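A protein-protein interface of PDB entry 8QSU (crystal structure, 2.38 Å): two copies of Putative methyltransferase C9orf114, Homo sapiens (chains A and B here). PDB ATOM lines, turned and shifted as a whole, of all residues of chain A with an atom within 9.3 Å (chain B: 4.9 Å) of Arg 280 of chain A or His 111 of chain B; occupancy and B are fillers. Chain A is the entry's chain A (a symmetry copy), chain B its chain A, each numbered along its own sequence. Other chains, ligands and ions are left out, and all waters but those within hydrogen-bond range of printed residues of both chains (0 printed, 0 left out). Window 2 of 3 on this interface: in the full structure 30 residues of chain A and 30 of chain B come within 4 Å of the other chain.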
ATOM      1  N   GLU A 222      25.061  10.269  29.391  1.00  0.00           N
ATOM      2  CA  GLU A 222      25.216  11.716  29.334  1.00  0.00           C
ATOM      3  C   GLU A 222      25.174  12.342  30.720  1.00  0.00           C
ATOM      4  O   GLU A 222      25.459  13.540  30.857  1.00  0.00           O
ATOM      5  CB  GLU A 222      24.140  12.346  28.432  1.00  0.00           C
ATOM      6  CG  GLU A 222      22.730  12.340  29.019  1.00  0.00           C
ATOM      7  CD  GLU A 222      21.637  12.357  27.954  1.00  0.00           C
ATOM      8  OE1 GLU A 222      20.870  13.345  27.899  1.00  0.00           O
ATOM      9  OE2 GLU A 222      21.542  11.379  27.176  1.00  0.00           O
ATOM     10  N   ARG A 223      24.854  11.553  31.748  1.00  0.00           N
ATOM     11  CA  ARG A 223      24.859  12.005  33.133  1.00  0.00           C
ATOM     12  C   ARG A 223      26.110  11.585  33.889  1.00  0.00           C
ATOM     13  O   ARG A 223      26.220  11.862  35.086  1.00  0.00           O
ATOM     14  CB  ARG A 223      23.626  11.474  33.860  1.00  0.00           C
ATOM     15  CG  ARG A 223      22.325  12.108  33.421  1.00  0.00           C
ATOM     16  CD  ARG A 223      21.160  11.325  33.992  1.00  0.00           C
ATOM     17  NE  ARG A 223      20.445  10.605  32.948  1.00  0.00           N
ATOM     18  CZ  ARG A 223      19.242  10.942  32.506  1.00  0.00           C
ATOM     19  NH1 ARG A 223      18.565  11.940  33.047  1.00  0.00           N
ATOM     20  NH2 ARG A 223      18.707  10.259  31.499  1.00  0.00           N
ATOM     21  N   LEU A 245      17.927   2.678  23.808  1.00  0.00           N
ATOM     22  CA  LEU A 245      17.103   3.869  23.670  1.00  0.00           C
ATOM     23  C   LEU A 245      16.841   4.535  25.019  1.00  0.00           C
ATOM     24  O   LEU A 245      16.953   5.760  25.150  1.00  0.00           O
ATOM     25  CB  LEU A 245      15.795   3.490  22.984  1.00  0.00           C
ATOM     26  CG  LEU A 245      14.806   4.626  22.787  1.00  0.00           C
ATOM     27  CD1 LEU A 245      15.510   5.782  22.094  1.00  0.00           C
ATOM     28  CD2 LEU A 245      13.609   4.151  21.981  1.00  0.00           C
ATOM     29  N   ASN A 272      30.435  10.518  30.827  1.00  0.00           N
ATOM     30  CA  ASN A 272      29.995  11.199  29.608  1.00  0.00           C
ATOM     31  C   ASN A 272      31.219  11.425  28.730  1.00  0.00           C
ATOM     32  O   ASN A 272      32.164  12.109  29.140  1.00  0.00           O
ATOM     33  CB  ASN A 272      29.330  12.530  29.978  1.00  0.00           C
ATOM     34  CG  ASN A 272      28.782  13.315  28.762  1.00  0.00           C
ATOM     35  OD1 ASN A 272      29.303  13.234  27.640  1.00  0.00           O
ATOM     36  ND2 ASN A 272      27.726  14.092  29.005  1.00  0.00           N
ATOM     37  N   CYS A 274      31.165  12.808  25.557  1.00  0.00           N
ATOM     38  CA  CYS A 274      30.993  13.868  24.557  1.00  0.00           C
ATOM     39  C   CYS A 274      30.489  15.085  25.304  1.00  0.00           C
ATOM     40  O   CYS A 274      29.270  15.302  25.437  1.00  0.00           O
ATOM     41  CB  CYS A 274      30.030  13.469  23.434  1.00  0.00           C
ATOM     42  SG  CYS A 274      30.312  14.202  21.725  1.00  0.00           S
ATOM     43  N   GLY A 276      29.186  18.660  25.818  1.00  0.00           N
ATOM     44  CA  GLY A 276      28.472  19.606  24.982  1.00  0.00           C
ATOM     45  C   GLY A 276      28.027  19.031  23.654  1.00  0.00           C
ATOM     46  O   GLY A 276      28.250  19.646  22.601  1.00  0.00           O
ATOM     47  N   GLN A 277      27.413  17.850  23.674  1.00  0.00           N
ATOM     48  CA  GLN A 277      26.884  17.294  22.438  1.00  0.00           C
ATOM     49  C   GLN A 277      25.908  18.273  21.783  1.00  0.00           C
ATOM     50  O   GLN A 277      25.229  19.057  22.455  1.00  0.00           O
ATOM     51  CB  GLN A 277      26.209  15.950  22.708  1.00  0.00           C
ATOM     52  CG  GLN A 277      25.328  15.929  23.943  1.00  0.00           C
ATOM     53  CD  GLN A 277      24.732  14.559  24.197  1.00  0.00           C
ATOM     54  OE1 GLN A 277      25.261  13.773  24.981  1.00  0.00           O
ATOM     55  NE2 GLN A 277      23.627  14.267  23.534  1.00  0.00           N
ATOM     56  N   GLY A 278      25.883  18.268  20.450  1.00  0.00           N
ATOM     57  CA  GLY A 278      24.991  19.139  19.699  1.00  0.00           C
ATOM     58  C   GLY A 278      23.670  18.513  19.324  1.00  0.00           C
ATOM     59  O   GLY A 278      22.800  19.193  18.775  1.00  0.00           O
ATOM     60  N   SER A 279      23.502  17.216  19.607  1.00  0.00           N
ATOM     61  CA  SER A 279      22.252  16.493  19.411  1.00  0.00           C
ATOM     62  C   SER A 279      21.738  15.999  20.761  1.00  0.00           C
ATOM     63  O   SER A 279      22.530  15.629  21.629  1.00  0.00           O
ATOM     64  CB  SER A 279      22.462  15.323  18.447  1.00  0.00           C
ATOM     65  OG  SER A 279      21.464  14.323  18.604  1.00  0.00           O
ATOM     66  N   ARG A 280      20.408  16.007  20.936  1.00  0.00           N
ATOM     67  CA  ARG A 280      19.793  15.584  22.197  1.00  0.00           C
ATOM     68  C   ARG A 280      20.224  14.180  22.613  1.00  0.00           C
ATOM     69  O   ARG A 280      20.318  13.883  23.809  1.00  0.00           O
ATOM     70  CB  ARG A 280      18.268  15.625  22.081  1.00  0.00           C
ATOM     71  CG  ARG A 280      17.580  16.708  22.912  1.00  0.00           C
ATOM     72  CD  ARG A 280      17.273  17.949  22.106  1.00  0.00           C
ATOM     73  NE  ARG A 280      16.160  17.786  21.170  1.00  0.00           N
ATOM     74  CZ  ARG A 280      15.608  18.791  20.498  1.00  0.00           C
ATOM     75  NH1 ARG A 280      16.011  20.035  20.672  1.00  0.00           N
ATOM     76  NH2 ARG A 280      14.637  18.537  19.623  1.00  0.00           N
ATOM     77  N   THR A 281      20.490  13.306  21.643  1.00  0.00           N
ATOM     78  CA  THR A 281      20.743  11.901  21.905  1.00  0.00           C
ATOM     79  C   THR A 281      21.818  11.384  20.967  1.00  0.00           C
ATOM     80  O   THR A 281      21.804  11.680  19.769  1.00  0.00           O
ATOM     81  CB  THR A 281      19.469  11.066  21.725  1.00  0.00           C
ATOM     82  OG1 THR A 281      18.833  11.434  20.489  1.00  0.00           O
ATOM     83  CG2 THR A 281      18.503  11.285  22.893  1.00  0.00           C
ATOM     84  N   ILE A 282      22.743  10.612  21.523  1.00  0.00           N
ATOM     85  CA  ILE A 282      23.735   9.879  20.754  1.00  0.00           C
ATOM     86  C   ILE A 282      23.281   8.429  20.715  1.00  0.00           C
ATOM     87  O   ILE A 282      23.157   7.778  21.760  1.00  0.00           O
ATOM     88  CB  ILE A 282      25.139  10.008  21.363  1.00  0.00           C
ATOM     89  CG1 ILE A 282      25.518  11.489  21.504  1.00  0.00           C
ATOM     90  CG2 ILE A 282      26.152   9.281  20.513  1.00  0.00           C
ATOM     91  CD1 ILE A 282      26.830  11.738  22.254  1.00  0.00           C
ATOM     92  N   ARG A 283      23.027   7.923  19.520  1.00  0.00           N
ATOM     93  CA  ARG A 283      22.619   6.537  19.405  1.00  0.00           C
ATOM     94  C   ARG A 283      23.769   5.612  19.792  1.00  0.00           C
ATOM     95  O   ARG A 283      24.952   5.989  19.753  1.00  0.00           O
ATOM     96  CB  ARG A 283      22.134   6.256  17.991  1.00  0.00           C
ATOM     97  CG  ARG A 283      21.163   7.321  17.517  1.00  0.00           C
ATOM     98  CD  ARG A 283      21.043   7.292  16.016  1.00  0.00           C
ATOM     99  NE  ARG A 283      20.690   5.953  15.564  1.00  0.00           N
ATOM    100  CZ  ARG A 283      19.443   5.513  15.505  1.00  0.00           C
ATOM    101  NH1 ARG A 283      18.426   6.299  15.816  1.00  0.00           N
ATOM    102  NH2 ARG A 283      19.211   4.258  15.116  1.00  0.00           N
ATOM    103  N   GLU A 286      26.569   5.101  17.512  1.00  0.00           N
ATOM    104  CA  GLU A 286      27.447   6.268  17.486  1.00  0.00           C
ATOM    105  C   GLU A 286      28.207   6.391  18.795  1.00  0.00           C
ATOM    106  O   GLU A 286      29.399   6.725  18.803  1.00  0.00           O
ATOM    107  CB  GLU A 286      26.649   7.558  17.220  1.00  0.00           C
ATOM    108  CG  GLU A 286      25.978   7.598  15.883  1.00  0.00           C
ATOM    109  CD  GLU A 286      24.738   8.437  15.915  1.00  0.00           C
ATOM    110  OE1 GLU A 286      24.252   8.702  17.043  1.00  0.00           O
ATOM    111  OE2 GLU A 286      24.247   8.815  14.816  1.00  0.00           O
ATOM    112  N   LEU B  80      18.359  17.892   6.532  1.00  0.00           N
ATOM    113  CA  LEU B  80      18.374  17.494   7.939  1.00  0.00           C
ATOM    114  C   LEU B  80      18.728  18.657   8.862  1.00  0.00           C
ATOM    115  O   LEU B  80      18.242  18.710   9.996  1.00  0.00           O
ATOM    116  CB  LEU B  80      19.358  16.341   8.167  1.00  0.00           C
ATOM    117  CG  LEU B  80      19.029  14.975   7.562  1.00  0.00           C
ATOM    118  CD1 LEU B  80      20.208  14.023   7.699  1.00  0.00           C
ATOM    119  CD2 LEU B  80      17.773  14.382   8.195  1.00  0.00           C
ATOM    120  N   GLU B  81      19.585  19.578   8.414  1.00  0.00           N
ATOM    121  CA  GLU B  81      19.893  20.745   9.238  1.00  0.00           C
ATOM    122  C   GLU B  81      18.660  21.609   9.452  1.00  0.00           C
ATOM    123  O   GLU B  81      18.484  22.202  10.520  1.00  0.00           O
ATOM    124  CB  GLU B  81      21.016  21.556   8.600  1.00  0.00           C
ATOM    125  CG  GLU B  81      21.596  22.634   9.508  1.00  0.00           C
ATOM    126  CD  GLU B  81      20.780  23.934   9.523  1.00  0.00           C
ATOM    127  OE1 GLU B  81      20.115  24.264   8.516  1.00  0.00           O
ATOM    128  OE2 GLU B  81      20.786  24.612  10.561  1.00  0.00           O
ATOM    129  N   CYS B  82      17.775  21.658   8.471  1.00  0.00           N
ATOM    130  CA  CYS B  82      16.693  22.634   8.485  1.00  0.00           C
ATOM    131  C   CYS B  82      15.575  22.208   9.429  1.00  0.00           C
ATOM    132  O   CYS B  82      15.005  21.129   9.247  1.00  0.00           O
ATOM    133  CB  CYS B  82      16.154  22.823   7.079  1.00  0.00           C
ATOM    134  SG  CYS B  82      14.738  23.938   6.967  1.00  0.00           S
ATOM    135  N   PRO B  83      15.217  23.032  10.442  1.00  0.00           N
ATOM    136  CA  PRO B  83      14.005  22.782  11.244  1.00  0.00           C
ATOM    137  C   PRO B  83      12.849  22.239  10.426  1.00  0.00           C
ATOM    138  O   PRO B  83      12.474  22.847   9.411  1.00  0.00           O
ATOM    139  CB  PRO B  83      13.654  24.175  11.793  1.00  0.00           C
ATOM    140  CG  PRO B  83      14.952  24.916  11.825  1.00  0.00           C
ATOM    141  CD  PRO B  83      15.858  24.320  10.780  1.00  0.00           C
ATOM    142  N   LEU B 106      18.319  15.114  13.508  1.00  0.00           N
ATOM    143  CA  LEU B 106      19.494  15.679  14.164  1.00  0.00           C
ATOM    144  C   LEU B 106      19.221  15.982  15.628  1.00  0.00           C
ATOM    145  O   LEU B 106      20.123  15.871  16.468  1.00  0.00           O
ATOM    146  CB  LEU B 106      19.948  16.939  13.431  1.00  0.00           C
ATOM    147  CG  LEU B 106      20.566  16.672  12.060  1.00  0.00           C
ATOM    148  CD1 LEU B 106      21.326  17.874  11.575  1.00  0.00           C
ATOM    149  CD2 LEU B 106      21.484  15.463  12.185  1.00  0.00           C
ATOM    150  N   ASP B 107      17.991  16.376  15.956  1.00  0.00           N
ATOM    151  CA  ASP B 107      17.596  16.649  17.344  1.00  0.00           C
ATOM    152  C   ASP B 107      18.446  17.752  17.976  1.00  0.00           C
ATOM    153  O   ASP B 107      18.754  17.716  19.177  1.00  0.00           O
ATOM    154  CB  ASP B 107      17.638  15.385  18.199  1.00  0.00           C
ATOM    155  CG  ASP B 107      16.413  14.511  17.999  1.00  0.00           C
ATOM    156  OD1 ASP B 107      16.467  13.291  18.321  1.00  0.00           O
ATOM    157  OD2 ASP B 107      15.390  15.055  17.544  1.00  0.00           O
ATOM    158  N   SER B 108      18.815  18.727  17.155  1.00  0.00           N
ATOM    159  CA  SER B 108      19.631  19.852  17.578  1.00  0.00           C
ATOM    160  C   SER B 108      18.781  20.917  18.268  1.00  0.00           C
ATOM    161  O   SER B 108      17.557  20.936  18.128  1.00  0.00           O
ATOM    162  CB  SER B 108      20.353  20.440  16.367  1.00  0.00           C
ATOM    163  OG  SER B 108      21.402  19.550  15.974  1.00  0.00           O
ATOM    164  N   PRO B 109      19.418  21.801  19.043  1.00  0.00           N
ATOM    165  CA  PRO B 109      18.648  22.793  19.820  1.00  0.00           C
ATOM    166  C   PRO B 109      17.703  23.658  19.001  1.00  0.00           C
ATOM    167  O   PRO B 109      16.714  24.141  19.558  1.00  0.00           O
ATOM    168  CB  PRO B 109      19.744  23.629  20.497  1.00  0.00           C
ATOM    169  CG  PRO B 109      20.899  22.647  20.642  1.00  0.00           C
ATOM    170  CD  PRO B 109      20.855  21.834  19.383  1.00  0.00           C
ATOM    171  N   HIS B 110      17.931  23.855  17.709  1.00  0.00           N
ATOM    172  CA  HIS B 110      16.946  24.612  16.928  1.00  0.00           C
ATOM    173  C   HIS B 110      15.889  23.719  16.286  1.00  0.00           C
ATOM    174  O   HIS B 110      15.043  24.225  15.552  1.00  0.00           O
ATOM    175  CB  HIS B 110      17.629  25.476  15.853  1.00  0.00           C
ATOM    176  CG  HIS B 110      18.457  24.692  14.883  1.00  0.00           C
ATOM    177  ND1 HIS B 110      19.462  23.832  15.285  1.00  0.00           N
ATOM    178  CD2 HIS B 110      18.442  24.644  13.532  1.00  0.00           C
ATOM    179  CE1 HIS B 110      20.028  23.291  14.222  1.00  0.00           C
ATOM    180  NE2 HIS B 110      19.418  23.753  13.146  1.00  0.00           N
ATOM    181  N   HIS B 111      15.907  22.410  16.556  1.00  0.00           N
ATOM    182  CA  HIS B 111      14.843  21.496  16.130  1.00  0.00           C
ATOM    183  C   HIS B 111      13.966  21.210  17.340  1.00  0.00           C
ATOM    184  O   HIS B 111      14.112  20.199  18.032  1.00  0.00           O
ATOM    185  CB  HIS B 111      15.422  20.207  15.558  1.00  0.00           C
ATOM    186  CG  HIS B 111      16.309  20.429  14.385  1.00  0.00           C
ATOM    187  ND1 HIS B 111      17.037  19.417  13.801  1.00  0.00           N
ATOM    188  CD2 HIS B 111      16.600  21.559  13.695  1.00  0.00           C
ATOM    189  CE1 HIS B 111      17.735  19.910  12.795  1.00  0.00           C
ATOM    190  NE2 HIS B 111      17.487  21.208  12.710  1.00  0.00           N
ATOM    191  N   MET B 112      13.038  22.116  17.595  1.00  0.00           N
ATOM    192  CA  MET B 112      12.177  21.938  18.741  1.00  0.00           C
ATOM    193  C   MET B 112      10.722  21.875  18.307  1.00  0.00           C
ATOM    194  O   MET B 112      10.397  22.229  17.171  1.00  0.00           O
ATOM    195  CB  MET B 112      12.413  23.052  19.755  1.00  0.00           C
ATOM    196  CG  MET B 112      11.577  24.303  19.544  1.00  0.00           C
ATOM    197  SD  MET B 112      12.312  25.559  18.241  1.00  0.00           S
ATOM    198  CE  MET B 112      13.925  26.088  19.186  1.00  0.00           C
ATOM    199  N   ARG B 113       9.867  21.371  19.202  1.00  0.00           N
ATOM    200  CA  ARG B 113       8.433  21.274  18.958  1.00  0.00           C
ATOM    201  C   ARG B 113       7.778  22.643  19.132  1.00  0.00           C
ATOM    202  O   ARG B 113       8.426  23.635  19.457  1.00  0.00           O
ATOM    203  CB  ARG B 113       7.795  20.259  19.906  1.00  0.00           C
ATOM    204  CG  ARG B 113       7.893  20.674  21.365  1.00  0.00           C
ATOM    205  CD  ARG B 113       7.208  19.726  22.324  1.00  0.00           C
ATOM    206  NE  ARG B 113       6.980  18.397  21.768  1.00  0.00           N
ATOM    207  CZ  ARG B 113       7.740  17.343  22.029  1.00  0.00           C
ATOM    208  NH1 ARG B 113       8.796  17.429  22.822  1.00  0.00           N
ATOM    209  NH2 ARG B 113       7.431  16.169  21.483  1.00  0.00           N
ATOM    210  N   GLU B 116       7.279  24.203  22.946  1.00  0.00           N
ATOM    211  CA  GLU B 116       8.585  24.269  23.598  1.00  0.00           C
ATOM    212  C   GLU B 116       9.003  25.734  23.656  1.00  0.00           C
ATOM    213  O   GLU B 116       9.318  26.333  22.622  1.00  0.00           O
ATOM    214  CB  GLU B 116       9.621  23.424  22.846  1.00  0.00           C
ATOM    215  CG  GLU B 116      10.248  22.278  23.650  1.00  0.00           C
ATOM    216  CD  GLU B 116      11.134  21.364  22.793  1.00  0.00           C
ATOM    217  OE1 GLU B 116      10.891  21.256  21.574  1.00  0.00           O
ATOM    218  OE2 GLU B 116      12.080  20.744  23.330  1.00  0.00           O
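The backbone carbonyl oxygen (O) of Leu 106 of chain B is in hydrogen-bond range of the side-chain hydroxyl (OG) of Ser 279 of chain A, 3.0 Å away. The backbone carbonyl oxygen (O) of Asp 107 of chain B lies within hydrogen-bond range of the backbone NH (N) of Arg 280 of chain A, 3.0 Å away. The side-chain hydroxyl (OG) of Ser 108 of chain B is in hydrogen-bond range of the backbone carbonyl oxygen (O) of Gly 278 of chain A (3.2 Å). O of Ser 108 of chain B lies within hydrogen-bond range of NH1 of Arg 280 of chain A (3.1 Å). The guanidinium group of Arg 280 of chain A sits close to the backbone carbonyl oxygen of His 111 of chain B.
O of Glu 81 of chain B is in hydrogen-bond range of NE2 of His 111 of chain B, at 2.6 Å. A ring nitrogen (NE2) of His 111 of chain B sits at hydrogen-bond distance from a ring nitrogen (NE2) of His 110 of chain B (3.2 Å). NE2 of Gln 277 of chain A is in hydrogen-bond range of O of Ser 279 of chain A. The backbone carbonyl oxygen of Arg 280 of chain A lies within hydrogen-bond range of the side-chain amide nitrogen of Gln 277 of chain A (3.3 Å). The side-chain hydroxyl (OG) of Ser 279 of chain A lies within hydrogen-bond range of the backbone carbonyl oxygen (O) of Thr 281 of chain A, at 2.9 Å.
Among the printed residues, pairs that only touch across the chains: Gly 278 of chain A with Pro 109 of chain B (3.3 Å), Thr 281 of chain A with Asp 107 of chain B (3.7 Å), Ser 279 of chain A with Asp 107 of chain B (3.7 Å) and Arg 280 of chain A with Pro 109 of chain B (3.9 Å).
Of chain A, only Arg 280 (2.4 Å) comes within 4 Å of His 111 of chain B. Printed residues of chain A within 4 Å of Asp 107 of chain B: Ser 279, Arg 280 and Thr 281. Ser 108 of chain B touches two residues of chain A. No residue of chain A comes within 4 Å of His 110 of chain B. No residue of chain A comes within 4 Å of Met 112 of chain B. Of the printed residues of chain B, Thr 281 of chain A touches Asp 107 (3.7 Å). Of the printed residues of chain B, Gly 278 of chain A touches Ser 108 (3.2 Å) and Pro 109 (3.3 Å). Printed residues of chain A within 4 Å of Pro 109 of chain B: Gly 278 and Arg 280. Of the printed residues of chain A, Leu 106 of chain B touches Ser 279 (3.0 Å). Of the printed residues of chain B, Ser 279 of chain A touches Leu 106 (3.0 Å) and Asp 107 (3.7 Å).
Of the 14 printed residues of chain A, 4 touch a printed residue of chain B. Among the printed residues, 9 pairs touch across the chains. Among the printed residues, no Asp or Glu carboxylate lies within 4 Å of a Lys or Arg side-chain nitrogen of the other chain.
No position is printed for both chains. Of the 9 pairs that touch across the chains among the printed residues, none has its exchanged pair printed and touching as well.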
